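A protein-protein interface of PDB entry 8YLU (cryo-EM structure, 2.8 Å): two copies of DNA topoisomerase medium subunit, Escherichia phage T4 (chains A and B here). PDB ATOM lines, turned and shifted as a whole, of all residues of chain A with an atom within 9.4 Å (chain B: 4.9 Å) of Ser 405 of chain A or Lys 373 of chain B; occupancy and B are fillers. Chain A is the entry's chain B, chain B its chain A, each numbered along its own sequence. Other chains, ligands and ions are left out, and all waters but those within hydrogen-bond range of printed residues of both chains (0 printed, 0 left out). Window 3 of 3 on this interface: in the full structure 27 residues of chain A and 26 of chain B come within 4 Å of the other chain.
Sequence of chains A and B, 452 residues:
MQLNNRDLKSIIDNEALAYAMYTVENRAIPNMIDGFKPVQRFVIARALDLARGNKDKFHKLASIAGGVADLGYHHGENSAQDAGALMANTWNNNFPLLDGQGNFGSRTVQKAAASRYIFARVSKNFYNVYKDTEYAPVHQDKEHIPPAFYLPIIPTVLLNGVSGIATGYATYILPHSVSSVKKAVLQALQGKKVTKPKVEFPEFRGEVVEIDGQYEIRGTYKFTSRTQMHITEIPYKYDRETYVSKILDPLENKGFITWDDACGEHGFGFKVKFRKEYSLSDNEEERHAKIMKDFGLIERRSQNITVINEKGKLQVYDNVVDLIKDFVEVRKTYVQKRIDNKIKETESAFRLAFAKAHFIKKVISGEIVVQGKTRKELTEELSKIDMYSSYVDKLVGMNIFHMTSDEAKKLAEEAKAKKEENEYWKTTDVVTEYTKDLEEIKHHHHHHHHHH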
ATOM      1  N   ILE A 360      19.985  30.178 -22.054  1.00  0.00           N
ATOM      2  CA  ILE A 360      20.557  28.981 -21.446  1.00  0.00           C
ATOM      3  C   ILE A 360      20.353  27.761 -22.337  1.00  0.00           C
ATOM      4  O   ILE A 360      21.263  26.939 -22.502  1.00  0.00           O
ATOM      5  CB  ILE A 360      19.980  28.770 -20.035  1.00  0.00           C
ATOM      6  CG1 ILE A 360      20.772  29.614 -19.042  1.00  0.00           C
ATOM      7  CG2 ILE A 360      20.025  27.301 -19.643  1.00  0.00           C
ATOM      8  CD1 ILE A 360      22.237  29.759 -19.425  1.00  0.00           C
ATOM      9  N   LYS A 361      19.162  27.615 -22.923  1.00  0.00           N
ATOM     10  CA  LYS A 361      18.933  26.505 -23.842  1.00  0.00           C
ATOM     11  C   LYS A 361      19.799  26.624 -25.089  1.00  0.00           C
ATOM     12  O   LYS A 361      20.152  25.608 -25.697  1.00  0.00           O
ATOM     13  CB  LYS A 361      17.456  26.432 -24.226  1.00  0.00           C
ATOM     14  CG  LYS A 361      16.708  25.276 -23.586  1.00  0.00           C
ATOM     15  CD  LYS A 361      15.328  25.109 -24.196  1.00  0.00           C
ATOM     16  CE  LYS A 361      15.013  23.643 -24.449  1.00  0.00           C
ATOM     17  NZ  LYS A 361      15.688  23.135 -25.675  1.00  0.00           N
ATOM     18  N   ILE A 364      23.456  25.236 -24.158  1.00  0.00           N
ATOM     19  CA  ILE A 364      23.552  23.783 -24.099  1.00  0.00           C
ATOM     20  C   ILE A 364      23.453  23.229 -25.513  1.00  0.00           C
ATOM     21  O   ILE A 364      22.352  23.083 -26.056  1.00  0.00           O
ATOM     22  CB  ILE A 364      22.458  23.185 -23.197  1.00  0.00           C
ATOM     23  CG1 ILE A 364      22.525  23.792 -21.796  1.00  0.00           C
ATOM     24  CG2 ILE A 364      22.582  21.673 -23.136  1.00  0.00           C
ATOM     25  CD1 ILE A 364      21.390  23.367 -20.898  1.00  0.00           C
ATOM     26  N   ILE A 400      27.312  29.322 -13.420  1.00  0.00           N
ATOM     27  CA  ILE A 400      27.548  28.088 -14.165  1.00  0.00           C
ATOM     28  C   ILE A 400      26.453  27.069 -13.879  1.00  0.00           C
ATOM     29  O   ILE A 400      26.047  26.309 -14.767  1.00  0.00           O
ATOM     30  CB  ILE A 400      28.950  27.537 -13.844  1.00  0.00           C
ATOM     31  CG1 ILE A 400      30.023  28.351 -14.569  1.00  0.00           C
ATOM     32  CG2 ILE A 400      29.067  26.072 -14.220  1.00  0.00           C
ATOM     33  CD1 ILE A 400      31.433  27.999 -14.156  1.00  0.00           C
ATOM     34  N   PHE A 401      25.942  27.040 -12.645  1.00  0.00           N
ATOM     35  CA  PHE A 401      24.878  26.099 -12.316  1.00  0.00           C
ATOM     36  C   PHE A 401      23.588  26.379 -13.076  1.00  0.00           C
ATOM     37  O   PHE A 401      22.702  25.518 -13.090  1.00  0.00           O
ATOM     38  CB  PHE A 401      24.646  26.068 -10.793  1.00  0.00           C
ATOM     39  CG  PHE A 401      24.172  27.375 -10.186  1.00  0.00           C
ATOM     40  CD1 PHE A 401      23.025  28.018 -10.623  1.00  0.00           C
ATOM     41  CD2 PHE A 401      24.890  27.952  -9.153  1.00  0.00           C
ATOM     42  CE1 PHE A 401      22.615  29.204 -10.052  1.00  0.00           C
ATOM     43  CE2 PHE A 401      24.481  29.138  -8.579  1.00  0.00           C
ATOM     44  CZ  PHE A 401      23.344  29.764  -9.029  1.00  0.00           C
ATOM     45  N   HIS A 402      23.461  27.549 -13.705  1.00  0.00           N
ATOM     46  CA  HIS A 402      22.343  27.801 -14.603  1.00  0.00           C
ATOM     47  C   HIS A 402      22.644  27.223 -15.976  1.00  0.00           C
ATOM     48  O   HIS A 402      22.458  27.899 -16.989  1.00  0.00           O
ATOM     49  CB  HIS A 402      22.081  29.303 -14.732  1.00  0.00           C
ATOM     50  CG  HIS A 402      21.306  29.890 -13.595  1.00  0.00           C
ATOM     51  ND1 HIS A 402      20.505  29.133 -12.769  1.00  0.00           N
ATOM     52  CD2 HIS A 402      21.210  31.164 -13.149  1.00  0.00           C
ATOM     53  CE1 HIS A 402      19.947  29.916 -11.863  1.00  0.00           C
ATOM     54  NE2 HIS A 402      20.360  31.153 -12.070  1.00  0.00           N
ATOM     55  N   MET A 403      23.097  25.974 -16.025  1.00  0.00           N
ATOM     56  CA  MET A 403      23.348  25.305 -17.292  1.00  0.00           C
ATOM     57  C   MET A 403      22.995  23.828 -17.251  1.00  0.00           C
ATOM     58  O   MET A 403      23.214  23.131 -18.246  1.00  0.00           O
ATOM     59  CB  MET A 403      24.819  25.479 -17.716  1.00  0.00           C
ATOM     60  CG  MET A 403      25.085  26.780 -18.464  1.00  0.00           C
ATOM     61  SD  MET A 403      26.742  26.938 -19.159  1.00  0.00           S
ATOM     62  CE  MET A 403      27.142  25.233 -19.516  1.00  0.00           C
ATOM     63  N   THR A 404      22.467  23.333 -16.141  1.00  0.00           N
ATOM     64  CA  THR A 404      21.971  21.973 -16.026  1.00  0.00           C
ATOM     65  C   THR A 404      20.470  21.957 -16.278  1.00  0.00           C
ATOM     66  O   THR A 404      19.788  22.976 -16.156  1.00  0.00           O
ATOM     67  CB  THR A 404      22.283  21.398 -14.642  1.00  0.00           C
ATOM     68  OG1 THR A 404      21.523  22.100 -13.651  1.00  0.00           O
ATOM     69  CG2 THR A 404      23.761  21.550 -14.330  1.00  0.00           C
ATOM     70  N   SER A 405      19.958  20.775 -16.630  1.00  0.00           N
ATOM     71  CA  SER A 405      18.545  20.655 -16.975  1.00  0.00           C
ATOM     72  C   SER A 405      17.651  21.081 -15.817  1.00  0.00           C
ATOM     73  O   SER A 405      16.630  21.752 -16.022  1.00  0.00           O
ATOM     74  CB  SER A 405      18.230  19.221 -17.397  1.00  0.00           C
ATOM     75  OG  SER A 405      19.151  18.765 -18.372  1.00  0.00           O
ATOM     76  N   ASP A 406      18.027  20.710 -14.591  1.00  0.00           N
ATOM     77  CA  ASP A 406      17.215  21.047 -13.427  1.00  0.00           C
ATOM     78  C   ASP A 406      17.076  22.554 -13.263  1.00  0.00           C
ATOM     79  O   ASP A 406      15.981  23.057 -12.988  1.00  0.00           O
ATOM     80  CB  ASP A 406      17.824  20.425 -12.170  1.00  0.00           C
ATOM     81  CG  ASP A 406      16.774  19.931 -11.199  1.00  0.00           C
ATOM     82  OD1 ASP A 406      15.818  19.264 -11.646  1.00  0.00           O
ATOM     83  OD2 ASP A 406      16.906  20.208  -9.989  1.00  0.00           O
ATOM     84  N   GLU A 407      18.172  23.291 -13.428  1.00  0.00           N
ATOM     85  CA  GLU A 407      18.129  24.742 -13.336  1.00  0.00           C
ATOM     86  C   GLU A 407      17.785  25.411 -14.658  1.00  0.00           C
ATOM     87  O   GLU A 407      17.533  26.622 -14.673  1.00  0.00           O
ATOM     88  CB  GLU A 407      19.467  25.282 -12.822  1.00  0.00           C
ATOM     89  CG  GLU A 407      19.605  25.247 -11.310  1.00  0.00           C
ATOM     90  CD  GLU A 407      18.984  26.455 -10.635  1.00  0.00           C
ATOM     91  OE1 GLU A 407      18.308  27.247 -11.323  1.00  0.00           O
ATOM     92  OE2 GLU A 407      19.172  26.613  -9.410  1.00  0.00           O
ATOM     93  N   ALA A 408      17.764  24.664 -15.762  1.00  0.00           N
ATOM     94  CA  ALA A 408      17.334  25.240 -17.031  1.00  0.00           C
ATOM     95  C   ALA A 408      15.817  25.252 -17.147  1.00  0.00           C
ATOM     96  O   ALA A 408      15.241  26.199 -17.692  1.00  0.00           O
ATOM     97  CB  ALA A 408      17.950  24.473 -18.201  1.00  0.00           C
ATOM     98  N   LYS A 409      15.152  24.209 -16.643  1.00  0.00           N
ATOM     99  CA  LYS A 409      13.693  24.197 -16.668  1.00  0.00           C
ATOM    100  C   LYS A 409      13.109  25.163 -15.646  1.00  0.00           C
ATOM    101  O   LYS A 409      11.998  25.670 -15.838  1.00  0.00           O
ATOM    102  CB  LYS A 409      13.170  22.779 -16.431  1.00  0.00           C
ATOM    103  CG  LYS A 409      13.229  22.313 -14.987  1.00  0.00           C
ATOM    104  CD  LYS A 409      12.534  20.974 -14.814  1.00  0.00           C
ATOM    105  CE  LYS A 409      13.003  19.969 -15.853  1.00  0.00           C
ATOM    106  NZ  LYS A 409      12.644  18.574 -15.478  1.00  0.00           N
ATOM    107  N   LYS A 410      13.839  25.434 -14.561  1.00  0.00           N
ATOM    108  CA  LYS A 410      13.364  26.399 -13.575  1.00  0.00           C
ATOM    109  C   LYS A 410      13.301  27.804 -14.157  1.00  0.00           C
ATOM    110  O   LYS A 410      12.416  28.583 -13.789  1.00  0.00           O
ATOM    111  CB  LYS A 410      14.260  26.375 -12.338  1.00  0.00           C
ATOM    112  CG  LYS A 410      13.497  26.369 -11.023  1.00  0.00           C
ATOM    113  CD  LYS A 410      14.348  25.831  -9.884  1.00  0.00           C
ATOM    114  CE  LYS A 410      14.751  24.386 -10.127  1.00  0.00           C
ATOM    115  NZ  LYS A 410      13.568  23.499 -10.311  1.00  0.00           N
ATOM    116  N   LEU A 411      14.218  28.144 -15.064  1.00  0.00           N
ATOM    117  CA  LEU A 411      14.162  29.447 -15.717  1.00  0.00           C
ATOM    118  C   LEU A 411      12.906  29.582 -16.573  1.00  0.00           C
ATOM    119  O   LEU A 411      12.233  30.620 -16.545  1.00  0.00           O
ATOM    120  CB  LEU A 411      15.415  29.658 -16.564  1.00  0.00           C
ATOM    121  CG  LEU A 411      16.622  30.252 -15.839  1.00  0.00           C
ATOM    122  CD1 LEU A 411      17.913  29.832 -16.521  1.00  0.00           C
ATOM    123  CD2 LEU A 411      16.509  31.764 -15.776  1.00  0.00           C
ATOM    124  N   ALA A 412      12.572  28.537 -17.334  1.00  0.00           N
ATOM    125  CA  ALA A 412      11.353  28.566 -18.134  1.00  0.00           C
ATOM    126  C   ALA A 412      10.113  28.614 -17.250  1.00  0.00           C
ATOM    127  O   ALA A 412       9.138  29.302 -17.576  1.00  0.00           O
ATOM    128  CB  ALA A 412      11.304  27.355 -19.064  1.00  0.00           C
ATOM    129  N   GLU A 413      10.127  27.883 -16.132  1.00  0.00           N
ATOM    130  CA  GLU A 413       9.001  27.933 -15.205  1.00  0.00           C
ATOM    131  C   GLU A 413       8.834  29.327 -14.614  1.00  0.00           C
ATOM    132  O   GLU A 413       7.710  29.819 -14.472  1.00  0.00           O
ATOM    133  CB  GLU A 413       9.184  26.897 -14.098  1.00  0.00           C
ATOM    134  CG  GLU A 413       8.848  25.477 -14.520  1.00  0.00           C
ATOM    135  CD  GLU A 413       8.430  24.608 -13.351  1.00  0.00           C
ATOM    136  OE1 GLU A 413       8.375  25.125 -12.216  1.00  0.00           O
ATOM    137  OE2 GLU A 413       8.157  23.409 -13.569  1.00  0.00           O
ATOM    138  N   VAL B 369      31.813  19.435 -18.835  1.00  0.00           N
ATOM    139  CA  VAL B 369      31.066  20.270 -19.766  1.00  0.00           C
ATOM    140  C   VAL B 369      29.974  21.085 -19.084  1.00  0.00           C
ATOM    141  O   VAL B 369      29.644  22.178 -19.575  1.00  0.00           O
ATOM    142  CB  VAL B 369      30.463  19.416 -20.903  1.00  0.00           C
ATOM    143  CG1 VAL B 369      29.819  20.292 -21.969  1.00  0.00           C
ATOM    144  CG2 VAL B 369      31.525  18.523 -21.517  1.00  0.00           C
ATOM    145  N   VAL B 370      29.428  20.619 -17.957  1.00  0.00           N
ATOM    146  CA  VAL B 370      28.314  21.261 -17.263  1.00  0.00           C
ATOM    147  C   VAL B 370      27.131  21.387 -18.217  1.00  0.00           C
ATOM    148  O   VAL B 370      26.483  22.436 -18.296  1.00  0.00           O
ATOM    149  CB  VAL B 370      28.715  22.628 -16.674  1.00  0.00           C
ATOM    150  CG1 VAL B 370      27.731  23.054 -15.598  1.00  0.00           C
ATOM    151  CG2 VAL B 370      30.121  22.571 -16.098  1.00  0.00           C
ATOM    152  N   GLN B 371      26.840  20.314 -18.947  1.00  0.00           N
ATOM    153  CA  GLN B 371      25.695  20.273 -19.843  1.00  0.00           C
ATOM    154  C   GLN B 371      25.094  18.877 -19.815  1.00  0.00           C
ATOM    155  O   GLN B 371      25.819  17.884 -19.715  1.00  0.00           O
ATOM    156  CB  GLN B 371      26.085  20.655 -21.276  1.00  0.00           C
ATOM    157  CG  GLN B 371      26.055  22.153 -21.546  1.00  0.00           C
ATOM    158  CD  GLN B 371      27.101  22.588 -22.553  1.00  0.00           C
ATOM    159  OE1 GLN B 371      27.793  23.586 -22.354  1.00  0.00           O
ATOM    160  NE2 GLN B 371      27.220  21.840 -23.643  1.00  0.00           N
ATOM    161  N   GLY B 372      23.770  18.809 -19.911  1.00  0.00           N
ATOM    162  CA  GLY B 372      23.075  17.537 -19.885  1.00  0.00           C
ATOM    163  C   GLY B 372      23.209  16.795 -18.571  1.00  0.00           C
ATOM    164  O   GLY B 372      23.483  15.591 -18.556  1.00  0.00           O
ATOM    165  N   LYS B 373      23.021  17.501 -17.460  1.00  0.00           N
ATOM    166  CA  LYS B 373      23.095  16.896 -16.138  1.00  0.00           C
ATOM    167  C   LYS B 373      22.174  17.672 -15.202  1.00  0.00           C
ATOM    168  O   LYS B 373      21.367  18.496 -15.640  1.00  0.00           O
ATOM    169  CB  LYS B 373      24.543  16.873 -15.635  1.00  0.00           C
ATOM    170  CG  LYS B 373      25.124  18.249 -15.355  1.00  0.00           C
ATOM    171  CD  LYS B 373      26.387  18.490 -16.157  1.00  0.00           C
ATOM    172  CE  LYS B 373      27.498  17.532 -15.755  1.00  0.00           C
ATOM    173  NZ  LYS B 373      28.790  17.870 -16.420  1.00  0.00           N
ATOM    174  N   THR B 374      22.294  17.401 -13.908  1.00  0.00           N
ATOM    175  CA  THR B 374      21.545  18.092 -12.868  1.00  0.00           C
ATOM    176  C   THR B 374      22.507  18.909 -12.011  1.00  0.00           C
ATOM    177  O   THR B 374      23.703  19.001 -12.295  1.00  0.00           O
ATOM    178  CB  THR B 374      20.755  17.099 -12.012  1.00  0.00           C
ATOM    179  OG1 THR B 374      21.650  16.131 -11.452  1.00  0.00           O
ATOM    180  CG2 THR B 374      19.711  16.385 -12.852  1.00  0.00           C
ATOM    181  N   ARG B 375      21.970  19.514 -10.951  1.00  0.00           N
ATOM    182  CA  ARG B 375      22.809  20.291 -10.046  1.00  0.00           C
ATOM    183  C   ARG B 375      23.372  19.427  -8.922  1.00  0.00           C
ATOM    184  O   ARG B 375      24.562  19.522  -8.601  1.00  0.00           O
ATOM    185  CB  ARG B 375      22.016  21.466  -9.473  1.00  0.00           C
ATOM    186  CG  ARG B 375      22.865  22.672  -9.103  1.00  0.00           C
ATOM    187  CD  ARG B 375      22.182  23.522  -8.045  1.00  0.00           C
ATOM    188  NE  ARG B 375      23.126  24.364  -7.322  1.00  0.00           N
ATOM    189  CZ  ARG B 375      22.883  25.613  -6.949  1.00  0.00           C
ATOM    190  NH1 ARG B 375      21.731  26.203  -7.218  1.00  0.00           N
ATOM    191  NH2 ARG B 375      23.821  26.287  -6.289  1.00  0.00           N
ATOM    192  N   LEU B 378      25.934  16.986 -10.371  1.00  0.00           N
ATOM    193  CA  LEU B 378      27.148  17.736 -10.681  1.00  0.00           C
ATOM    194  C   LEU B 378      27.934  18.046  -9.415  1.00  0.00           C
ATOM    195  O   LEU B 378      29.168  17.957  -9.403  1.00  0.00           O
ATOM    196  CB  LEU B 378      26.797  19.028 -11.416  1.00  0.00           C
ATOM    197  CG  LEU B 378      27.982  19.882 -11.867  1.00  0.00           C
ATOM    198  CD1 LEU B 378      28.955  19.063 -12.700  1.00  0.00           C
ATOM    199  CD2 LEU B 378      27.504  21.098 -12.629  1.00  0.00           C
ATOM    200  N   GLU B 381      29.664  14.869  -8.378  1.00  0.00           N
ATOM    201  CA  GLU B 381      30.782  14.580  -9.271  1.00  0.00           C
ATOM    202  C   GLU B 381      31.970  15.486  -8.973  1.00  0.00           C
ATOM    203  O   GLU B 381      33.125  15.045  -9.018  1.00  0.00           O
ATOM    204  CB  GLU B 381      30.336  14.727 -10.725  1.00  0.00           C
ATOM    205  CG  GLU B 381      31.461  14.654 -11.743  1.00  0.00           C
ATOM    206  CD  GLU B 381      31.040  13.961 -13.024  1.00  0.00           C
ATOM    207  OE1 GLU B 381      29.929  14.247 -13.517  1.00  0.00           O
ATOM    208  OE2 GLU B 381      31.820  13.133 -13.538  1.00  0.00           O
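O of Lys 373 of chain B sits at hydrogen-bond distance from N of Ser 405 of chain A. The guanidinium group (NH1) of Arg 375 of chain B lies within salt-bridge range of the side-chain carboxylate (OE2) of Glu 407 of chain A, at 3.4 Å. The backbone carbonyl oxygen (O) of Met 403 of chain A lies close to the backbone carbonyl oxygen (O) of Val 370 of chain B.
OE1 of Glu 407 of chain A sits close to ND1 of His 402 of chain A, at 3.2 Å.
Among the printed residues, merely in contact across the chains: Ile 364 of chain A with Gln 371 of chain B (3.8 Å), Ile 400 of chain A with Val 370 of chain B (3.6 Å), Phe 401 of chain A with Arg 375 of chain B (3.5 Å), Met 403 of chain A with Val 369 of chain B (3.9 Å), Met 403 of chain A with Gln 371 of chain B (3.3 Å), Thr 404 of chain A with Lys 373 of chain B (3.2 Å), Thr 404 of chain A with Thr 374 of chain B (3.3 Å) and Thr 404 of chain A with Arg 375 of chain B (3.8 Å).
Of the printed residues of chain B, Ile 400 of chain A touches Val 370 (3.6 Å). Val 370 of chain B touches two residues of chain A. Of chain A, only Thr 404 (3.2 Å) and Ser 405 (2.9 Å) come within 4 Å of Lys 373 of chain B. Of the printed residues of chain A, Arg 375 of chain B touches Phe 401, Thr 404 and Glu 407. The nearest residue of chain B that does not touch Ser 405 of chain A is Gly 372 of chain B (4.4 Å). The nearest residue of chain A that does not touch Lys 373 of chain B is Asp 406 of chain A (4.1 Å). The nearest printed residue of chain B that does not touch Glu 407 of chain A is Lys 373 of chain B (6.2 Å).
Of the 17 printed residues of chain A, 7 touch a printed residue of chain B. Printed residues of chain A that touch a printed residue of chain B: Ile 364, Ile 400, Phe 401, Met 403, Thr 404, Ser 405 and Glu 407. Hydrophobic or aromatic side chains of chain A within 4 Å of the printed part of chain B: Ile 364, Ile 400, Phe 401 and Met 403. Hydrophobic or aromatic side chains of chain B within 4 Å of the printed part of chain A: Val 370. Along chain B the printed residues that touch a printed residue of chain A span positions 369 to 375. Among the printed residues, 11 pairs touch across the chains. Among the printed residues, Asp or Glu carboxylates within 4 Å of a Lys or Arg side-chain nitrogen of the other chain: Glu 407 of chain A with Arg 375 of chain B (3.4 Å).
No position is printed for both chains. Of the 11 pairs that touch across the chains among the printed residues, none has its exchanged pair printed and touching as well.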
